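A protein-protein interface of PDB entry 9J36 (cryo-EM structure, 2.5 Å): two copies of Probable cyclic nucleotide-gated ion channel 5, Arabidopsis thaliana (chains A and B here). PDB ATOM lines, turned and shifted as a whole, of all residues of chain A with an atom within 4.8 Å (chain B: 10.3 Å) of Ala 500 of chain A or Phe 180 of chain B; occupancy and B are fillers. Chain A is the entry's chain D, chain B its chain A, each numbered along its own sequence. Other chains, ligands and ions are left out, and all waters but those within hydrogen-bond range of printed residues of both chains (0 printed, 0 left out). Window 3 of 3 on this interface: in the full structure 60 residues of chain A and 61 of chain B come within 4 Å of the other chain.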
ATOM      1  N   CYS A 498      26.187 -17.622  20.231  1.00  0.00           N
ATOM      2  CA  CYS A 498      26.024 -16.807  21.421  1.00  0.00           C
ATOM      3  C   CYS A 498      24.615 -16.742  21.987  1.00  0.00           C
ATOM      4  O   CYS A 498      24.348 -15.837  22.770  1.00  0.00           O
ATOM      5  CB  CYS A 498      26.473 -15.368  21.135  1.00  0.00           C
ATOM      6  SG  CYS A 498      28.030 -15.186  20.263  1.00  0.00           S
ATOM      7  N   LEU A 499      23.695 -17.632  21.617  1.00  0.00           N
ATOM      8  CA  LEU A 499      22.329 -17.459  22.109  1.00  0.00           C
ATOM      9  C   LEU A 499      22.133 -18.117  23.463  1.00  0.00           C
ATOM     10  O   LEU A 499      21.463 -17.558  24.336  1.00  0.00           O
ATOM     11  CB  LEU A 499      21.318 -18.020  21.122  1.00  0.00           C
ATOM     12  CG  LEU A 499      19.860 -17.681  21.385  1.00  0.00           C
ATOM     13  CD1 LEU A 499      19.699 -16.202  21.198  1.00  0.00           C
ATOM     14  CD2 LEU A 499      18.957 -18.442  20.450  1.00  0.00           C
ATOM     15  N   ALA A 500      22.682 -19.315  23.647  1.00  0.00           N
ATOM     16  CA  ALA A 500      22.612 -20.026  24.916  1.00  0.00           C
ATOM     17  C   ALA A 500      23.348 -19.304  26.034  1.00  0.00           C
ATOM     18  O   ALA A 500      22.928 -19.393  27.190  1.00  0.00           O
ATOM     19  CB  ALA A 500      23.167 -21.442  24.757  1.00  0.00           C
ATOM     20  N   LEU A 501      24.417 -18.582  25.713  1.00  0.00           N
ATOM     21  CA  LEU A 501      25.104 -17.739  26.678  1.00  0.00           C
ATOM     22  C   LEU A 501      24.268 -16.554  27.136  1.00  0.00           C
ATOM     23  O   LEU A 501      24.217 -16.277  28.338  1.00  0.00           O
ATOM     24  CB  LEU A 501      26.416 -17.222  26.086  1.00  0.00           C
ATOM     25  CG  LEU A 501      27.521 -18.244  25.835  1.00  0.00           C
ATOM     26  CD1 LEU A 501      28.695 -17.570  25.177  1.00  0.00           C
ATOM     27  CD2 LEU A 501      27.950 -18.915  27.121  1.00  0.00           C
ATOM     28  N   VAL A 502      23.617 -15.848  26.214  1.00  0.00           N
ATOM     29  CA  VAL A 502      22.797 -14.703  26.591  1.00  0.00           C
ATOM     30  C   VAL A 502      21.503 -15.150  27.264  1.00  0.00           C
ATOM     31  O   VAL A 502      21.010 -14.482  28.181  1.00  0.00           O
ATOM     32  CB  VAL A 502      22.549 -13.829  25.350  1.00  0.00           C
ATOM     33  CG1 VAL A 502      21.749 -12.604  25.683  1.00  0.00           C
ATOM     34  CG2 VAL A 502      23.868 -13.375  24.795  1.00  0.00           C
ATOM     35  N   ARG A 503      20.972 -16.314  26.894  1.00  0.00           N
ATOM     36  CA  ARG A 503      19.743 -16.827  27.487  1.00  0.00           C
ATOM     37  C   ARG A 503      19.997 -17.658  28.740  1.00  0.00           C
ATOM     38  O   ARG A 503      19.190 -18.533  29.080  1.00  0.00           O
ATOM     39  CB  ARG A 503      18.957 -17.635  26.455  1.00  0.00           C
ATOM     40  CG  ARG A 503      17.976 -16.798  25.655  1.00  0.00           C
ATOM     41  CD  ARG A 503      17.085 -17.665  24.786  1.00  0.00           C
ATOM     42  NE  ARG A 503      16.202 -18.517  25.577  1.00  0.00           N
ATOM     43  CZ  ARG A 503      16.321 -19.838  25.659  1.00  0.00           C
ATOM     44  NH1 ARG A 503      17.292 -20.457  25.001  1.00  0.00           N
ATOM     45  NH2 ARG A 503      15.474 -20.538  26.399  1.00  0.00           N
ATOM     46  N   ARG A 504      21.111 -17.415  29.425  1.00  0.00           N
ATOM     47  CA  ARG A 504      21.301 -17.856  30.792  1.00  0.00           C
ATOM     48  C   ARG A 504      21.348 -16.688  31.763  1.00  0.00           C
ATOM     49  O   ARG A 504      21.238 -16.904  32.974  1.00  0.00           O
ATOM     50  CB  ARG A 504      22.585 -18.691  30.919  1.00  0.00           C
ATOM     51  CG  ARG A 504      22.519 -19.754  31.994  1.00  0.00           C
ATOM     52  CD  ARG A 504      23.797 -20.563  32.065  1.00  0.00           C
ATOM     53  NE  ARG A 504      23.846 -21.374  33.278  1.00  0.00           N
ATOM     54  CZ  ARG A 504      24.887 -22.113  33.644  1.00  0.00           C
ATOM     55  NH1 ARG A 504      25.976 -22.150  32.891  1.00  0.00           N
ATOM     56  NH2 ARG A 504      24.840 -22.815  34.768  1.00  0.00           N
ATOM     57  N   ILE A 547      31.234 -16.635  29.698  1.00  0.00           N
ATOM     58  CA  ILE A 547      32.390 -17.523  29.633  1.00  0.00           C
ATOM     59  C   ILE A 547      32.114 -18.668  28.668  1.00  0.00           C
ATOM     60  O   ILE A 547      31.082 -19.339  28.754  1.00  0.00           O
ATOM     61  CB  ILE A 547      32.750 -18.050  31.030  1.00  0.00           C
ATOM     62  CG1 ILE A 547      32.810 -16.907  32.038  1.00  0.00           C
ATOM     63  CG2 ILE A 547      34.069 -18.785  31.003  1.00  0.00           C
ATOM     64  CD1 ILE A 547      33.837 -15.857  31.725  1.00  0.00           C
ATOM     65  N   ILE A 548      33.037 -18.886  27.742  1.00  0.00           N
ATOM     66  CA  ILE A 548      33.007 -20.022  26.836  1.00  0.00           C
ATOM     67  C   ILE A 548      33.740 -21.209  27.426  1.00  0.00           C
ATOM     68  O   ILE A 548      33.196 -22.304  27.534  1.00  0.00           O
ATOM     69  CB  ILE A 548      33.629 -19.631  25.479  1.00  0.00           C
ATOM     70  CG1 ILE A 548      32.805 -18.581  24.758  1.00  0.00           C
ATOM     71  CG2 ILE A 548      33.830 -20.840  24.599  1.00  0.00           C
ATOM     72  CD1 ILE A 548      33.616 -17.902  23.709  1.00  0.00           C
ATOM     73  N   GLU A 572      32.486 -22.926  32.657  1.00  0.00           N
ATOM     74  CA  GLU A 572      31.997 -22.870  31.284  1.00  0.00           C
ATOM     75  C   GLU A 572      30.483 -22.724  31.222  1.00  0.00           C
ATOM     76  O   GLU A 572      29.744 -23.673  31.499  1.00  0.00           O
ATOM     77  CB  GLU A 572      32.417 -24.141  30.549  1.00  0.00           C
ATOM     78  CG  GLU A 572      33.909 -24.277  30.314  1.00  0.00           C
ATOM     79  CD  GLU A 572      34.674 -24.929  31.461  1.00  0.00           C
ATOM     80  OE1 GLU A 572      34.182 -24.925  32.609  1.00  0.00           O
ATOM     81  OE2 GLU A 572      35.785 -25.440  31.210  1.00  0.00           O
ATOM     82  N   GLY A 573      30.023 -21.534  30.835  1.00  0.00           N
ATOM     83  CA  GLY A 573      28.619 -21.257  30.622  1.00  0.00           C
ATOM     84  C   GLY A 573      28.087 -20.122  31.467  1.00  0.00           C
ATOM     85  O   GLY A 573      27.140 -19.447  31.054  1.00  0.00           O
ATOM     86  N   ALA B 174      31.779 -32.342  18.412  1.00  0.00           N
ATOM     87  CA  ALA B 174      30.702 -32.278  17.432  1.00  0.00           C
ATOM     88  C   ALA B 174      29.982 -30.934  17.530  1.00  0.00           C
ATOM     89  O   ALA B 174      29.934 -30.342  18.616  1.00  0.00           O
ATOM     90  CB  ALA B 174      29.734 -33.445  17.651  1.00  0.00           C
ATOM     91  N   PRO B 175      29.428 -30.410  16.433  1.00  0.00           N
ATOM     92  CA  PRO B 175      28.793 -29.089  16.496  1.00  0.00           C
ATOM     93  C   PRO B 175      27.425 -29.134  17.164  1.00  0.00           C
ATOM     94  O   PRO B 175      26.577 -29.974  16.854  1.00  0.00           O
ATOM     95  CB  PRO B 175      28.672 -28.682  15.023  1.00  0.00           C
ATOM     96  CG  PRO B 175      28.665 -29.936  14.279  1.00  0.00           C
ATOM     97  CD  PRO B 175      29.471 -30.927  15.052  1.00  0.00           C
ATOM     98  N   SER B 176      27.217 -28.192  18.085  1.00  0.00           N
ATOM     99  CA  SER B 176      25.949 -28.009  18.780  1.00  0.00           C
ATOM    100  C   SER B 176      25.929 -26.632  19.428  1.00  0.00           C
ATOM    101  O   SER B 176      26.983 -26.042  19.674  1.00  0.00           O
ATOM    102  CB  SER B 176      25.716 -29.090  19.848  1.00  0.00           C
ATOM    103  OG  SER B 176      25.499 -30.364  19.262  1.00  0.00           O
ATOM    104  N   SER B 177      24.723 -26.130  19.697  1.00  0.00           N
ATOM    105  CA  SER B 177      24.558 -24.860  20.391  1.00  0.00           C
ATOM    106  C   SER B 177      24.203 -25.036  21.861  1.00  0.00           C
ATOM    107  O   SER B 177      23.997 -24.038  22.561  1.00  0.00           O
ATOM    108  CB  SER B 177      23.480 -24.012  19.700  1.00  0.00           C
ATOM    109  OG  SER B 177      22.176 -24.426  20.067  1.00  0.00           O
ATOM    110  N   ARG B 178      24.142 -26.279  22.339  1.00  0.00           N
ATOM    111  CA  ARG B 178      23.857 -26.611  23.730  1.00  0.00           C
ATOM    112  C   ARG B 178      25.105 -26.485  24.603  1.00  0.00           C
ATOM    113  O   ARG B 178      25.015 -26.283  25.821  1.00  0.00           O
ATOM    114  CB  ARG B 178      23.279 -28.031  23.782  1.00  0.00           C
ATOM    115  CG  ARG B 178      23.044 -28.664  25.154  1.00  0.00           C
ATOM    116  CD  ARG B 178      23.009 -30.184  25.053  1.00  0.00           C
ATOM    117  NE  ARG B 178      24.299 -30.778  25.403  1.00  0.00           N
ATOM    118  CZ  ARG B 178      24.723 -31.963  24.974  1.00  0.00           C
ATOM    119  NH1 ARG B 178      25.912 -32.421  25.343  1.00  0.00           N
ATOM    120  NH2 ARG B 178      23.968 -32.685  24.156  1.00  0.00           N
ATOM    121  N   VAL B 179      26.272 -26.483  23.969  1.00  0.00           N
ATOM    122  CA  VAL B 179      27.528 -26.887  24.590  1.00  0.00           C
ATOM    123  C   VAL B 179      28.095 -25.862  25.569  1.00  0.00           C
ATOM    124  O   VAL B 179      28.756 -26.245  26.545  1.00  0.00           O
ATOM    125  CB  VAL B 179      28.553 -27.235  23.486  1.00  0.00           C
ATOM    126  CG1 VAL B 179      28.039 -28.380  22.667  1.00  0.00           C
ATOM    127  CG2 VAL B 179      28.787 -26.058  22.538  1.00  0.00           C
ATOM    128  N   PHE B 180      27.891 -24.565  25.276  1.00  0.00           N
ATOM    129  CA  PHE B 180      28.517 -23.379  25.880  1.00  0.00           C
ATOM    130  C   PHE B 180      30.034 -23.303  25.693  1.00  0.00           C
ATOM    131  O   PHE B 180      30.644 -22.315  26.105  1.00  0.00           O
ATOM    132  CB  PHE B 180      28.235 -23.266  27.387  1.00  0.00           C
ATOM    133  CG  PHE B 180      26.783 -23.210  27.745  1.00  0.00           C
ATOM    134  CD1 PHE B 180      26.135 -24.339  28.216  1.00  0.00           C
ATOM    135  CD2 PHE B 180      26.079 -22.021  27.668  1.00  0.00           C
ATOM    136  CE1 PHE B 180      24.801 -24.292  28.571  1.00  0.00           C
ATOM    137  CE2 PHE B 180      24.750 -21.962  28.026  1.00  0.00           C
ATOM    138  CZ  PHE B 180      24.108 -23.099  28.477  1.00  0.00           C
ATOM    139  N   GLY B 181      30.651 -24.313  25.080  1.00  0.00           N
ATOM    140  CA  GLY B 181      32.092 -24.475  25.101  1.00  0.00           C
ATOM    141  C   GLY B 181      32.689 -25.055  23.835  1.00  0.00           C
ATOM    142  O   GLY B 181      33.717 -25.737  23.900  1.00  0.00           O
ATOM    143  N   ARG B 182      32.013 -24.842  22.703  1.00  0.00           N
ATOM    144  CA  ARG B 182      32.407 -25.132  21.314  1.00  0.00           C
ATOM    145  C   ARG B 182      32.380 -26.610  20.942  1.00  0.00           C
ATOM    146  O   ARG B 182      32.996 -26.972  19.932  1.00  0.00           O
ATOM    147  CB  ARG B 182      33.794 -24.568  20.947  1.00  0.00           C
ATOM    148  CG  ARG B 182      33.985 -23.085  21.257  1.00  0.00           C
ATOM    149  CD  ARG B 182      33.515 -22.209  20.120  1.00  0.00           C
ATOM    150  NE  ARG B 182      32.062 -22.094  20.047  1.00  0.00           N
ATOM    151  CZ  ARG B 182      31.345 -21.209  20.726  1.00  0.00           C
ATOM    152  NH1 ARG B 182      31.947 -20.341  21.519  1.00  0.00           N
ATOM    153  NH2 ARG B 182      30.026 -21.190  20.606  1.00  0.00           N
ATOM    154  N   GLY B 183      31.696 -27.470  21.696  1.00  0.00           N
ATOM    155  CA  GLY B 183      31.558 -28.853  21.282  1.00  0.00           C
ATOM    156  C   GLY B 183      31.280 -29.880  22.364  1.00  0.00           C
ATOM    157  O   GLY B 183      31.665 -29.707  23.527  1.00  0.00           O
ATOM    158  N   GLU B 184      30.598 -30.958  21.973  1.00  0.00           N
ATOM    159  CA  GLU B 184      30.309 -32.083  22.857  1.00  0.00           C
ATOM    160  C   GLU B 184      31.494 -33.039  22.824  1.00  0.00           C
ATOM    161  O   GLU B 184      32.134 -33.198  21.784  1.00  0.00           O
ATOM    162  CB  GLU B 184      29.048 -32.809  22.400  1.00  0.00           C
ATOM    163  CG  GLU B 184      27.772 -32.007  22.464  1.00  0.00           C
ATOM    164  CD  GLU B 184      26.592 -32.747  21.879  1.00  0.00           C
ATOM    165  OE1 GLU B 184      26.802 -33.840  21.309  1.00  0.00           O
ATOM    166  OE2 GLU B 184      25.456 -32.244  21.978  1.00  0.00           O
ATOM    167  N   LEU B 185      31.784 -33.684  23.950  1.00  0.00           N
ATOM    168  CA  LEU B 185      32.681 -34.834  23.938  1.00  0.00           C
ATOM    169  C   LEU B 185      31.867 -36.117  24.049  1.00  0.00           C
ATOM    170  O   LEU B 185      30.985 -36.238  24.902  1.00  0.00           O
ATOM    171  CB  LEU B 185      33.711 -34.750  25.071  1.00  0.00           C
ATOM    172  CG  LEU B 185      35.017 -33.964  24.908  1.00  0.00           C
ATOM    173  CD1 LEU B 185      34.782 -32.463  24.761  1.00  0.00           C
ATOM    174  CD2 LEU B 185      35.959 -34.248  26.075  1.00  0.00           C
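O of Ile 548 of chain A sits close to O of Phe 180 of chain B.
The backbone carbonyl oxygen (O) of Ile 547 of chain A lies within hydrogen-bond range of the backbone NH (N) of Gly 573 of chain A (3.2 Å).
The backbone carbonyl oxygen (O) of Gly 573 of chain A sits close to the guanidinium group (NH1) of Arg 504 of chain A.
CB of Ala 500 of chain A touches O of Ser 177 of chain B, at 3.5 Å.
O of Ala 500 of chain A touches CE2 of Phe 180 of chain B, at 3.3 Å.
Leu 501 of chain A touches Phe 180 of chain B (CD2 to CD2, 3.7 Å).
Gly 181 of chain B touches Ile 548 of chain A.
CG2 of Ile 548 of chain A touches NH1 of Arg 182 of chain B, 3.6 Å away.
CA of Gly 573 of chain A touches CB of Phe 180 of chain B, 3.8 Å away.
Ala 500 of chain A touches just these residues of chain B: Ser 177 and Phe 180.
Printed residues of chain A within 4 Å of Phe 180 of chain B: Ala 500, Leu 501, Ile 548 and Gly 573.
No residue of chain B comes within 4 Å of Leu 499 of chain A.
Leu 501 of chain A touches just one residue of chain B: Phe 180.
Ile 548 of chain A touches just these residues of chain B: Phe 180 (2.9 Å), Gly 181 (3.4 Å) and Arg 182 (3.6 Å).
Gly 573 of chain A touches just one residue of chain B: Phe 180.
Printed residues of chain A within 4 Å of Gly 181 of chain B: Ile 548.
Of the printed residues of chain A, Ser 177 of chain B touches Ala 500 (3.5 Å).
Of the printed residues of chain A, Arg 182 of chain B touches Ile 548 (3.6 Å).
Cys 498 of chain A touches none of the printed residues of chain B.
The nearest residue of chain B that does not touch Ala 500 of chain A is Arg 178 of chain B (5.3 Å).
The nearest printed residue of chain A that does not touch Gly 181 of chain B is Glu 572 of chain A (5.5 Å).
Of the 12 printed residues of chain B, 4 touch a printed residue of chain A.
Hydrophobic or aromatic side chains of chain B that line the printed part of chain A: Phe 180.
Hydrophobic or aromatic side chains of chain A that line the printed part of chain B: Ala 500, Leu 501 and Ile 548.
Among the printed residues, 7 pairs touch across the chains.
No position is printed for both chains.
Of the 7 pairs that touch across the chains among the printed residues, none has its exchanged pair printed and touching as well.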
